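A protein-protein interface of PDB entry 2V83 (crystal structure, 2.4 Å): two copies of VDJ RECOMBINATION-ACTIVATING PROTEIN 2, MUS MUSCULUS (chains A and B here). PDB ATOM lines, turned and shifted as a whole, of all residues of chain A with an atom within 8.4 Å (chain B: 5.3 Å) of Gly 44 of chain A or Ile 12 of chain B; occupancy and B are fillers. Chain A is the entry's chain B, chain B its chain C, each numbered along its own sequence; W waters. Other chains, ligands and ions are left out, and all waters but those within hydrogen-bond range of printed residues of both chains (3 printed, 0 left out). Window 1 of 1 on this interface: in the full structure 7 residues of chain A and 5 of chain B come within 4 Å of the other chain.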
ATOM      1  N   TYR A  40     -10.608 -12.824 -16.059  1.00  0.00           N
ATOM      2  CA  TYR A  40     -10.719 -13.087 -14.631  1.00  0.00           C
ATOM      3  C   TYR A  40      -9.429 -13.550 -13.941  1.00  0.00           C
ATOM      4  O   TYR A  40      -8.751 -14.481 -14.396  1.00  0.00           O
ATOM      5  CB  TYR A  40     -11.821 -14.124 -14.411  1.00  0.00           C
ATOM      6  CG  TYR A  40     -12.113 -14.448 -12.965  1.00  0.00           C
ATOM      7  CD1 TYR A  40     -12.779 -13.537 -12.145  1.00  0.00           C
ATOM      8  CD2 TYR A  40     -11.755 -15.686 -12.424  1.00  0.00           C
ATOM      9  CE1 TYR A  40     -13.088 -13.855 -10.825  1.00  0.00           C
ATOM     10  CE2 TYR A  40     -12.059 -16.014 -11.105  1.00  0.00           C
ATOM     11  CZ  TYR A  40     -12.725 -15.097 -10.313  1.00  0.00           C
ATOM     12  OH  TYR A  40     -13.043 -15.432  -9.018  1.00  0.00           O
ATOM     13  N   CYS A  41      -9.095 -12.883 -12.840  1.00  0.00           N
ATOM     14  CA  CYS A  41      -7.923 -13.248 -12.055  1.00  0.00           C
ATOM     15  C   CYS A  41      -8.434 -14.101 -10.885  1.00  0.00           C
ATOM     16  O   CYS A  41      -9.394 -13.722 -10.200  1.00  0.00           O
ATOM     17  CB  CYS A  41      -7.212 -12.000 -11.524  1.00  0.00           C
ATOM     18  SG  CYS A  41      -5.801 -12.370 -10.425  1.00  0.00           S
ATOM     19  N   SER A  42      -7.790 -15.244 -10.661  1.00  0.00           N
ATOM     20  CA  SER A  42      -8.186 -16.166  -9.600  1.00  0.00           C
ATOM     21  C   SER A  42      -7.541 -15.901  -8.237  1.00  0.00           C
ATOM     22  O   SER A  42      -7.624 -16.740  -7.342  1.00  0.00           O
ATOM     23  CB  SER A  42      -7.876 -17.599 -10.034  1.00  0.00           C
ATOM     24  OG  SER A  42      -8.530 -17.910 -11.250  1.00  0.00           O
ATOM     25  N   HIS A  43      -6.899 -14.747  -8.079  1.00  0.00           N
ATOM     26  CA  HIS A  43      -6.251 -14.408  -6.815  1.00  0.00           C
ATOM     27  C   HIS A  43      -7.256 -14.118  -5.700  1.00  0.00           C
ATOM     28  O   HIS A  43      -8.270 -13.454  -5.923  1.00  0.00           O
ATOM     29  CB  HIS A  43      -5.362 -13.185  -6.991  1.00  0.00           C
ATOM     30  CG  HIS A  43      -4.781 -12.689  -5.704  1.00  0.00           C
ATOM     31  ND1 HIS A  43      -3.744 -13.328  -5.060  1.00  0.00           N
ATOM     32  CD2 HIS A  43      -5.122 -11.640  -4.920  1.00  0.00           C
ATOM     33  CE1 HIS A  43      -3.471 -12.695  -3.935  1.00  0.00           C
ATOM     34  NE2 HIS A  43      -4.293 -11.666  -3.827  1.00  0.00           N
ATOM     35  N   GLY A  44      -6.963 -14.593  -4.494  1.00  0.00           N
ATOM     36  CA  GLY A  44      -7.870 -14.369  -3.384  1.00  0.00           C
ATOM     37  C   GLY A  44      -9.288 -14.769  -3.755  1.00  0.00           C
ATOM     38  O   GLY A  44      -9.509 -15.859  -4.288  1.00  0.00           O
ATOM     39  N   ASP A  45     -10.251 -13.892  -3.484  1.00  0.00           N
ATOM     40  CA  ASP A  45     -11.643 -14.176  -3.811  1.00  0.00           C
ATOM     41  C   ASP A  45     -11.931 -13.904  -5.290  1.00  0.00           C
ATOM     42  O   ASP A  45     -13.048 -14.102  -5.762  1.00  0.00           O
ATOM     43  CB  ASP A  45     -12.585 -13.339  -2.940  1.00  0.00           C
ATOM     44  CG  ASP A  45     -12.354 -13.550  -1.448  1.00  0.00           C
ATOM     45  OD1 ASP A  45     -11.951 -14.664  -1.044  1.00  0.00           O
ATOM     46  OD2 ASP A  45     -12.596 -12.599  -0.674  1.00  0.00           O
ATOM     47  N   GLY A  46     -10.915 -13.442  -6.013  1.00  0.00           N
ATOM     48  CA  GLY A  46     -11.074 -13.170  -7.427  1.00  0.00           C
ATOM     49  C   GLY A  46     -11.425 -11.737  -7.765  1.00  0.00           C
ATOM     50  O   GLY A  46     -11.778 -10.944  -6.899  1.00  0.00           O
ATOM     51  N   HIS A  47     -11.303 -11.403  -9.041  1.00  0.00           N
ATOM     52  CA  HIS A  47     -11.630 -10.074  -9.530  1.00  0.00           C
ATOM     53  C   HIS A  47     -11.394 -10.019 -11.031  1.00  0.00           C
ATOM     54  O   HIS A  47     -10.678 -10.856 -11.596  1.00  0.00           O
ATOM     55  CB  HIS A  47     -10.798  -8.990  -8.827  1.00  0.00           C
ATOM     56  CG  HIS A  47      -9.341  -9.011  -9.171  1.00  0.00           C
ATOM     57  ND1 HIS A  47      -8.681  -7.910  -9.667  1.00  0.00           N
ATOM     58  CD2 HIS A  47      -8.410  -9.988  -9.062  1.00  0.00           C
ATOM     59  CE1 HIS A  47      -7.406  -8.204  -9.848  1.00  0.00           C
ATOM     60  NE2 HIS A  47      -7.215  -9.458  -9.488  1.00  0.00           N
ATOM     61  N   TYR A  72      -3.662 -15.120 -13.505  1.00  0.00           N
ATOM     62  CA  TYR A  72      -3.365 -14.275 -12.368  1.00  0.00           C
ATOM     63  C   TYR A  72      -2.875 -12.992 -13.016  1.00  0.00           C
ATOM     64  O   TYR A  72      -2.007 -13.036 -13.889  1.00  0.00           O
ATOM     65  CB  TYR A  72      -2.282 -14.915 -11.488  1.00  0.00           C
ATOM     66  CG  TYR A  72      -2.747 -16.191 -10.816  1.00  0.00           C
ATOM     67  CD1 TYR A  72      -2.804 -17.394 -11.520  1.00  0.00           C
ATOM     68  CD2 TYR A  72      -3.221 -16.175  -9.505  1.00  0.00           C
ATOM     69  CE1 TYR A  72      -3.327 -18.541 -10.938  1.00  0.00           C
ATOM     70  CE2 TYR A  72      -3.750 -17.316  -8.914  1.00  0.00           C
ATOM     71  CZ  TYR A  72      -3.804 -18.497  -9.637  1.00  0.00           C
ATOM     72  OH  TYR A  72      -4.356 -19.621  -9.058  1.00  0.00           O
ATOM     73  N   HIS A  76      -0.879  -9.738  -9.174  1.00  0.00           N
ATOM     74  CA  HIS A  76      -0.861 -10.884  -8.270  1.00  0.00           C
ATOM     75  C   HIS A  76      -0.048 -12.115  -8.663  1.00  0.00           C
ATOM     76  O   HIS A  76       0.304 -12.917  -7.800  1.00  0.00           O
ATOM     77  CB  HIS A  76      -2.293 -11.335  -8.018  1.00  0.00           C
ATOM     78  CG  HIS A  76      -3.167 -10.272  -7.443  1.00  0.00           C
ATOM     79  ND1 HIS A  76      -4.402  -9.962  -7.968  1.00  0.00           N
ATOM     80  CD2 HIS A  76      -3.010  -9.482  -6.355  1.00  0.00           C
ATOM     81  CE1 HIS A  76      -4.971  -9.029  -7.226  1.00  0.00           C
ATOM     82  NE2 HIS A  76      -4.148  -8.722  -6.240  1.00  0.00           N
ATOM     83  N   ILE A  79       2.840 -13.456  -6.449  1.00  0.00           N
ATOM     84  CA  ILE A  79       2.615 -13.672  -5.041  1.00  0.00           C
ATOM     85  C   ILE A  79       2.698 -15.174  -4.830  1.00  0.00           C
ATOM     86  O   ILE A  79       1.939 -15.928  -5.430  1.00  0.00           O
ATOM     87  CB  ILE A  79       1.235 -13.133  -4.636  1.00  0.00           C
ATOM     88  CG1 ILE A  79       1.222 -11.609  -4.813  1.00  0.00           C
ATOM     89  CG2 ILE A  79       0.917 -13.520  -3.207  1.00  0.00           C
ATOM     90  CD1 ILE A  79      -0.135 -10.950  -4.631  1.00  0.00           C
ATOM     91  N   ALA A  80       3.653 -15.606  -4.012  1.00  0.00           N
ATOM     92  CA  ALA A  80       3.832 -17.021  -3.728  1.00  0.00           C
ATOM     93  C   ALA A  80       2.441 -17.579  -3.520  1.00  0.00           C
ATOM     94  O   ALA A  80       1.775 -17.283  -2.531  1.00  0.00           O
ATOM     95  CB  ALA A  80       4.677 -17.212  -2.479  1.00  0.00           C
ATOM     96  N   ARG A  81       1.985 -18.367  -4.474  1.00  0.00           N
ATOM     97  CA  ARG A  81       0.658 -18.934  -4.389  1.00  0.00           C
ATOM     98  C   ARG A  81       0.682 -20.413  -4.037  1.00  0.00           C
ATOM     99  O   ARG A  81       0.259 -21.266  -4.825  1.00  0.00           O
ATOM    100  CB  ARG A  81      -0.076 -18.719  -5.706  1.00  0.00           C
ATOM    101  CG  ARG A  81      -1.304 -19.573  -5.824  1.00  0.00           C
ATOM    102  CD  ARG A  81      -1.965 -19.377  -7.149  1.00  0.00           C
ATOM    103  NE  ARG A  81      -1.088 -18.686  -8.080  1.00  0.00           N
ATOM    104  CZ  ARG A  81      -0.414 -19.276  -9.056  1.00  0.00           C
ATOM    105  NH1 ARG A  81      -0.511 -20.581  -9.243  1.00  0.00           N
ATOM    106  NH2 ARG A  81       0.360 -18.551  -9.844  1.00  0.00           N
ATOM    107  N   ALA A  82       1.182 -20.714  -2.851  1.00  0.00           N
ATOM    108  CA  ALA A  82       1.236 -22.078  -2.386  1.00  0.00           C
ATOM    109  C   ALA A  82      -0.010 -22.283  -1.544  1.00  0.00           C
ATOM    110  O   ALA A  82      -0.833 -23.154  -1.906  1.00  0.00           O
ATOM    111  CB  ALA A  82       2.490 -22.280  -1.539  1.00  0.00           C
ATOM    112  OXT ALA A  82      -0.144 -21.550  -0.544  1.00  0.00           O
ATOM    113  N   PHE B   8      -8.722  -8.566  -1.327  1.00  0.00           N
ATOM    114  CA  PHE B   8      -9.146  -9.779  -1.996  1.00  0.00           C
ATOM    115  C   PHE B   8      -9.543 -10.949  -1.120  1.00  0.00           C
ATOM    116  O   PHE B   8      -9.431 -12.105  -1.525  1.00  0.00           O
ATOM    117  CB  PHE B   8      -8.068 -10.204  -2.999  1.00  0.00           C
ATOM    118  CG  PHE B   8      -7.711  -9.124  -3.974  1.00  0.00           C
ATOM    119  CD1 PHE B   8      -6.738  -8.177  -3.663  1.00  0.00           C
ATOM    120  CD2 PHE B   8      -8.401  -9.006  -5.174  1.00  0.00           C
ATOM    121  CE1 PHE B   8      -6.461  -7.123  -4.536  1.00  0.00           C
ATOM    122  CE2 PHE B   8      -8.133  -7.956  -6.051  1.00  0.00           C
ATOM    123  CZ  PHE B   8      -7.162  -7.013  -5.730  1.00  0.00           C
ATOM    124  N   GLY B   9     -10.009 -10.654   0.084  1.00  0.00           N
ATOM    125  CA  GLY B   9     -10.452 -11.723   0.955  1.00  0.00           C
ATOM    126  C   GLY B   9      -9.584 -12.150   2.116  1.00  0.00           C
ATOM    127  O   GLY B   9      -8.477 -11.659   2.329  1.00  0.00           O
ATOM    128  N   TYR B  10     -10.118 -13.107   2.863  1.00  0.00           N
ATOM    129  CA  TYR B  10      -9.469 -13.653   4.041  1.00  0.00           C
ATOM    130  C   TYR B  10      -8.906 -15.046   3.821  1.00  0.00           C
ATOM    131  O   TYR B  10      -8.279 -15.614   4.715  1.00  0.00           O
ATOM    132  CB  TYR B  10     -10.479 -13.709   5.184  1.00  0.00           C
ATOM    133  CG  TYR B  10     -10.942 -12.351   5.629  1.00  0.00           C
ATOM    134  CD1 TYR B  10     -11.908 -11.646   4.914  1.00  0.00           C
ATOM    135  CD2 TYR B  10     -10.357 -11.736   6.731  1.00  0.00           C
ATOM    136  CE1 TYR B  10     -12.276 -10.355   5.285  1.00  0.00           C
ATOM    137  CE2 TYR B  10     -10.712 -10.452   7.109  1.00  0.00           C
ATOM    138  CZ  TYR B  10     -11.669  -9.765   6.382  1.00  0.00           C
ATOM    139  OH  TYR B  10     -11.996  -8.482   6.748  1.00  0.00           O
ATOM    140  N   TRP B  11      -9.104 -15.585   2.623  1.00  0.00           N
ATOM    141  CA  TRP B  11      -8.675 -16.946   2.332  1.00  0.00           C
ATOM    142  C   TRP B  11      -7.406 -17.162   1.525  1.00  0.00           C
ATOM    143  O   TRP B  11      -7.151 -18.263   1.040  1.00  0.00           O
ATOM    144  CB  TRP B  11      -9.853 -17.670   1.703  1.00  0.00           C
ATOM    145  CG  TRP B  11     -11.084 -17.386   2.496  1.00  0.00           C
ATOM    146  CD1 TRP B  11     -12.069 -16.484   2.198  1.00  0.00           C
ATOM    147  CD2 TRP B  11     -11.413 -17.929   3.777  1.00  0.00           C
ATOM    148  NE1 TRP B  11     -12.988 -16.434   3.217  1.00  0.00           N
ATOM    149  CE2 TRP B  11     -12.609 -17.312   4.200  1.00  0.00           C
ATOM    150  CE3 TRP B  11     -10.808 -18.879   4.614  1.00  0.00           C
ATOM    151  CZ2 TRP B  11     -13.218 -17.615   5.421  1.00  0.00           C
ATOM    152  CZ3 TRP B  11     -11.412 -19.181   5.828  1.00  0.00           C
ATOM    153  CH2 TRP B  11     -12.605 -18.549   6.220  1.00  0.00           C
ATOM    154  N   ILE B  12      -6.607 -16.115   1.391  1.00  0.00           N
ATOM    155  CA  ILE B  12      -5.344 -16.212   0.678  1.00  0.00           C
ATOM    156  C   ILE B  12      -4.364 -16.989   1.554  1.00  0.00           C
ATOM    157  O   ILE B  12      -4.557 -17.093   2.764  1.00  0.00           O
ATOM    158  CB  ILE B  12      -4.750 -14.813   0.436  1.00  0.00           C
ATOM    159  CG1 ILE B  12      -4.940 -13.953   1.694  1.00  0.00           C
ATOM    160  CG2 ILE B  12      -5.410 -14.161  -0.766  1.00  0.00           C
ATOM    161  CD1 ILE B  12      -3.656 -13.499   2.350  1.00  0.00           C
ATOM    162  N   THR B  13      -3.332 -17.557   0.946  1.00  0.00           N
ATOM    163  CA  THR B  13      -2.317 -18.255   1.721  1.00  0.00           C
ATOM    164  C   THR B  13      -1.324 -17.123   1.991  1.00  0.00           C
ATOM    165  O   THR B  13      -0.529 -16.758   1.124  1.00  0.00           O
ATOM    166  CB  THR B  13      -1.659 -19.389   0.910  1.00  0.00           C
ATOM    167  OG1 THR B  13      -1.090 -18.856  -0.290  1.00  0.00           O
ATOM    168  CG2 THR B  13      -2.694 -20.450   0.548  1.00  0.00           C
ATOM    169  N   CYS B  14      -1.406 -16.555   3.193  1.00  0.00           N
ATOM    170  CA  CYS B  14      -0.581 -15.413   3.591  1.00  0.00           C
ATOM    171  C   CYS B  14       0.932 -15.608   3.655  1.00  0.00           C
ATOM    172  O   CYS B  14       1.684 -14.674   3.370  1.00  0.00           O
ATOM    173  CB  CYS B  14      -1.074 -14.863   4.939  1.00  0.00           C
ATOM    174  SG  CYS B  14      -0.767 -15.921   6.384  1.00  0.00           S
ATOM    175  N   CYS B  18       1.331 -20.842   5.683  1.00  0.00           N
ATOM    176  CA  CYS B  18      -0.118 -20.659   5.745  1.00  0.00           C
ATOM    177  C   CYS B  18      -0.889 -21.943   5.996  1.00  0.00           C
ATOM    178  O   CYS B  18      -0.884 -22.877   5.190  1.00  0.00           O
ATOM    179  CB  CYS B  18      -0.646 -19.980   4.482  1.00  0.00           C
ATOM    180  SG  CYS B  18      -2.320 -19.351   4.720  1.00  0.00           S
ATOM    181  N   VAL B  20      -4.309 -21.847   6.948  1.00  0.00           N
ATOM    182  CA  VAL B  20      -5.729 -21.589   6.721  1.00  0.00           C
ATOM    183  C   VAL B  20      -6.387 -22.174   5.466  1.00  0.00           C
ATOM    184  O   VAL B  20      -6.007 -21.855   4.342  1.00  0.00           O
ATOM    185  CB  VAL B  20      -5.981 -20.066   6.732  1.00  0.00           C
ATOM    186  CG1 VAL B  20      -7.450 -19.770   6.505  1.00  0.00           C
ATOM    187  CG2 VAL B  20      -5.512 -19.482   8.053  1.00  0.00           C
ATOM    188  N   MET B  38      -6.847 -10.917  10.635  1.00  0.00           N
ATOM    189  CA  MET B  38      -5.679 -10.516   9.885  1.00  0.00           C
ATOM    190  C   MET B  38      -5.102  -9.219  10.408  1.00  0.00           C
ATOM    191  O   MET B  38      -5.753  -8.457  11.127  1.00  0.00           O
ATOM    192  CB  MET B  38      -6.000 -10.395   8.400  1.00  0.00           C
ATOM    193  CG  MET B  38      -6.309 -11.735   7.757  1.00  0.00           C
ATOM    194  SD  MET B  38      -6.642 -11.625   6.002  1.00  0.00           S
ATOM    195  CE  MET B  38      -5.046 -11.943   5.308  1.00  0.00           C
ATOM    196  N   TRP B  48      -1.457  -8.537   3.710  1.00  0.00           N
ATOM    197  CA  TRP B  48      -2.226  -8.951   4.864  1.00  0.00           C
ATOM    198  C   TRP B  48      -1.803 -10.368   5.192  1.00  0.00           C
ATOM    199  O   TRP B  48      -1.529 -11.169   4.295  1.00  0.00           O
ATOM    200  CB  TRP B  48      -3.727  -8.905   4.583  1.00  0.00           C
ATOM    201  CG  TRP B  48      -4.293  -7.517   4.560  1.00  0.00           C
ATOM    202  CD1 TRP B  48      -4.287  -6.644   3.512  1.00  0.00           C
ATOM    203  CD2 TRP B  48      -4.935  -6.837   5.645  1.00  0.00           C
ATOM    204  NE1 TRP B  48      -4.887  -5.464   3.875  1.00  0.00           N
ATOM    205  CE2 TRP B  48      -5.294  -5.554   5.178  1.00  0.00           C
ATOM    206  CE3 TRP B  48      -5.243  -7.190   6.966  1.00  0.00           C
ATOM    207  CZ2 TRP B  48      -5.944  -4.618   5.992  1.00  0.00           C
ATOM    208  CZ3 TRP B  48      -5.890  -6.257   7.774  1.00  0.00           C
ATOM    209  CH2 TRP B  48      -6.234  -4.987   7.280  1.00  0.00           C
ATOM    210  N   HIS B  50      -2.446 -13.753   8.165  1.00  0.00           N
ATOM    211  CA  HIS B  50      -3.308 -14.308   9.207  1.00  0.00           C
ATOM    212  C   HIS B  50      -2.612 -14.213  10.553  1.00  0.00           C
ATOM    213  O   HIS B  50      -1.422 -14.518  10.676  1.00  0.00           O
ATOM    214  CB  HIS B  50      -3.632 -15.774   8.916  1.00  0.00           C
ATOM    215  CG  HIS B  50      -4.346 -15.990   7.619  1.00  0.00           C
ATOM    216  ND1 HIS B  50      -3.903 -16.888   6.674  1.00  0.00           N
ATOM    217  CD2 HIS B  50      -5.487 -15.455   7.123  1.00  0.00           C
ATOM    218  CE1 HIS B  50      -4.741 -16.903   5.654  1.00  0.00           C
ATOM    219  NE2 HIS B  50      -5.711 -16.043   5.901  1.00  0.00           N
HETATM  220  O   HOH W   1      -9.433 -14.649  -0.084  1.00  0.00           O
HETATM  221  O   HOH W   2     -12.628  -9.771  -1.827  1.00  0.00           O
HETATM  222  O   HOH W   3     -12.832 -12.693   2.105  1.00  0.00           O
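Gly 44 of chain A touches just these residues of chain B: Phe 8 (3.3 Å) and Ile 12 (3.6 Å). Printed residues of chain B within 4 Å of Asp 45 of chain A: Phe 8 (2.8 Å), Gly 9 (2.8 Å) and Trp 11 (3.7 Å). Printed residues of chain B within 4 Å of Ala 80 of chain A: Thr 13 (3.96 Å). Of the printed residues of chain B, Ala 82 of chain A touches Thr 13 (2.9 Å). Of the printed residues of chain A, Trp 11 of chain B touches Asp 45. Of the printed residues of chain A, Ile 12 of chain B touches His 43 (3.99 Å) and Gly 44 (3.6 Å). Of chain A, only Ala 80 (3.96 Å) and Ala 82 (2.9 Å) come within 4 Å of Thr 13 of chain B. The nearest printed residue of chain B that does not touch Gly 44 of chain A is Gly 9 of chain B (5.5 Å). The nearest printed residue of chain A that does not touch Ile 12 of chain B is Asp 45 of chain A (5.6 Å). The nearest printed residue of chain A that does not touch Phe 8 of chain B is Gly 46 of chain A (4.3 Å).
The backbone carbonyl oxygen (O) of Ile 12 of chain B sits close to the side-chain sulfur (SG) of Cys 18 of chain B, 3.7 Å away. SG of Cys 41 of chain A lies close to N of His 43 of chain A.
OXT of Ala 82 of chain A is in hydrogen-bond range of OG1 of Thr 13 of chain B (2.9 Å). The backbone carbonyl oxygen (O) of Phe 8 of chain B lies within hydrogen-bond range of the backbone NH (N) of Asp 45 of chain A. OD2 of Asp 45 of chain A lies close to N of Gly 9 of chain B.
Water W1 lies within hydrogen-bond range of the side-chain carboxylate (OD1) of Asp 45 of chain A, the backbone NH (N) of Trp 11 of chain B, the backbone carbonyl oxygen (O) of Phe 8 of chain B and the backbone NH (N) of Tyr 10 of chain B. Water W3 lies within hydrogen-bond range of OD2 of Asp 45 of chain A and N of Tyr 10 of chain B. Water W2 lies within hydrogen-bond range of OD2 of Asp 45 of chain A (3.1 Å) and N of Gly 9 of chain B (3.4 Å).
Among the printed residues, merely in contact across the chains: His 76 of chain A with Phe 8 of chain B (3.3 Å), Gly 44 of chain A with Phe 8 of chain B (3.3 Å), His 47 of chain A with Phe 8 of chain B (3.5 Å), Gly 44 of chain A with Ile 12 of chain B (3.6 Å), Asp 45 of chain A with Trp 11 of chain B (3.7 Å), His 43 of chain A with Phe 8 of chain B (3.7 Å), Ala 80 of chain A with Thr 13 of chain B (3.96 Å) and His 43 of chain A with Ile 12 of chain B (3.99 Å).
Hydrophobic or aromatic side chains of chain B that line the printed part of chain A: Phe 8, Trp 11 and Ile 12. Of the 14 printed residues of chain A, 7 touch a printed residue of chain B.
No position is printed for both chains. Of the 11 pairs that touch across the chains among the printed residues, none has its exchanged pair printed and touching as well.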
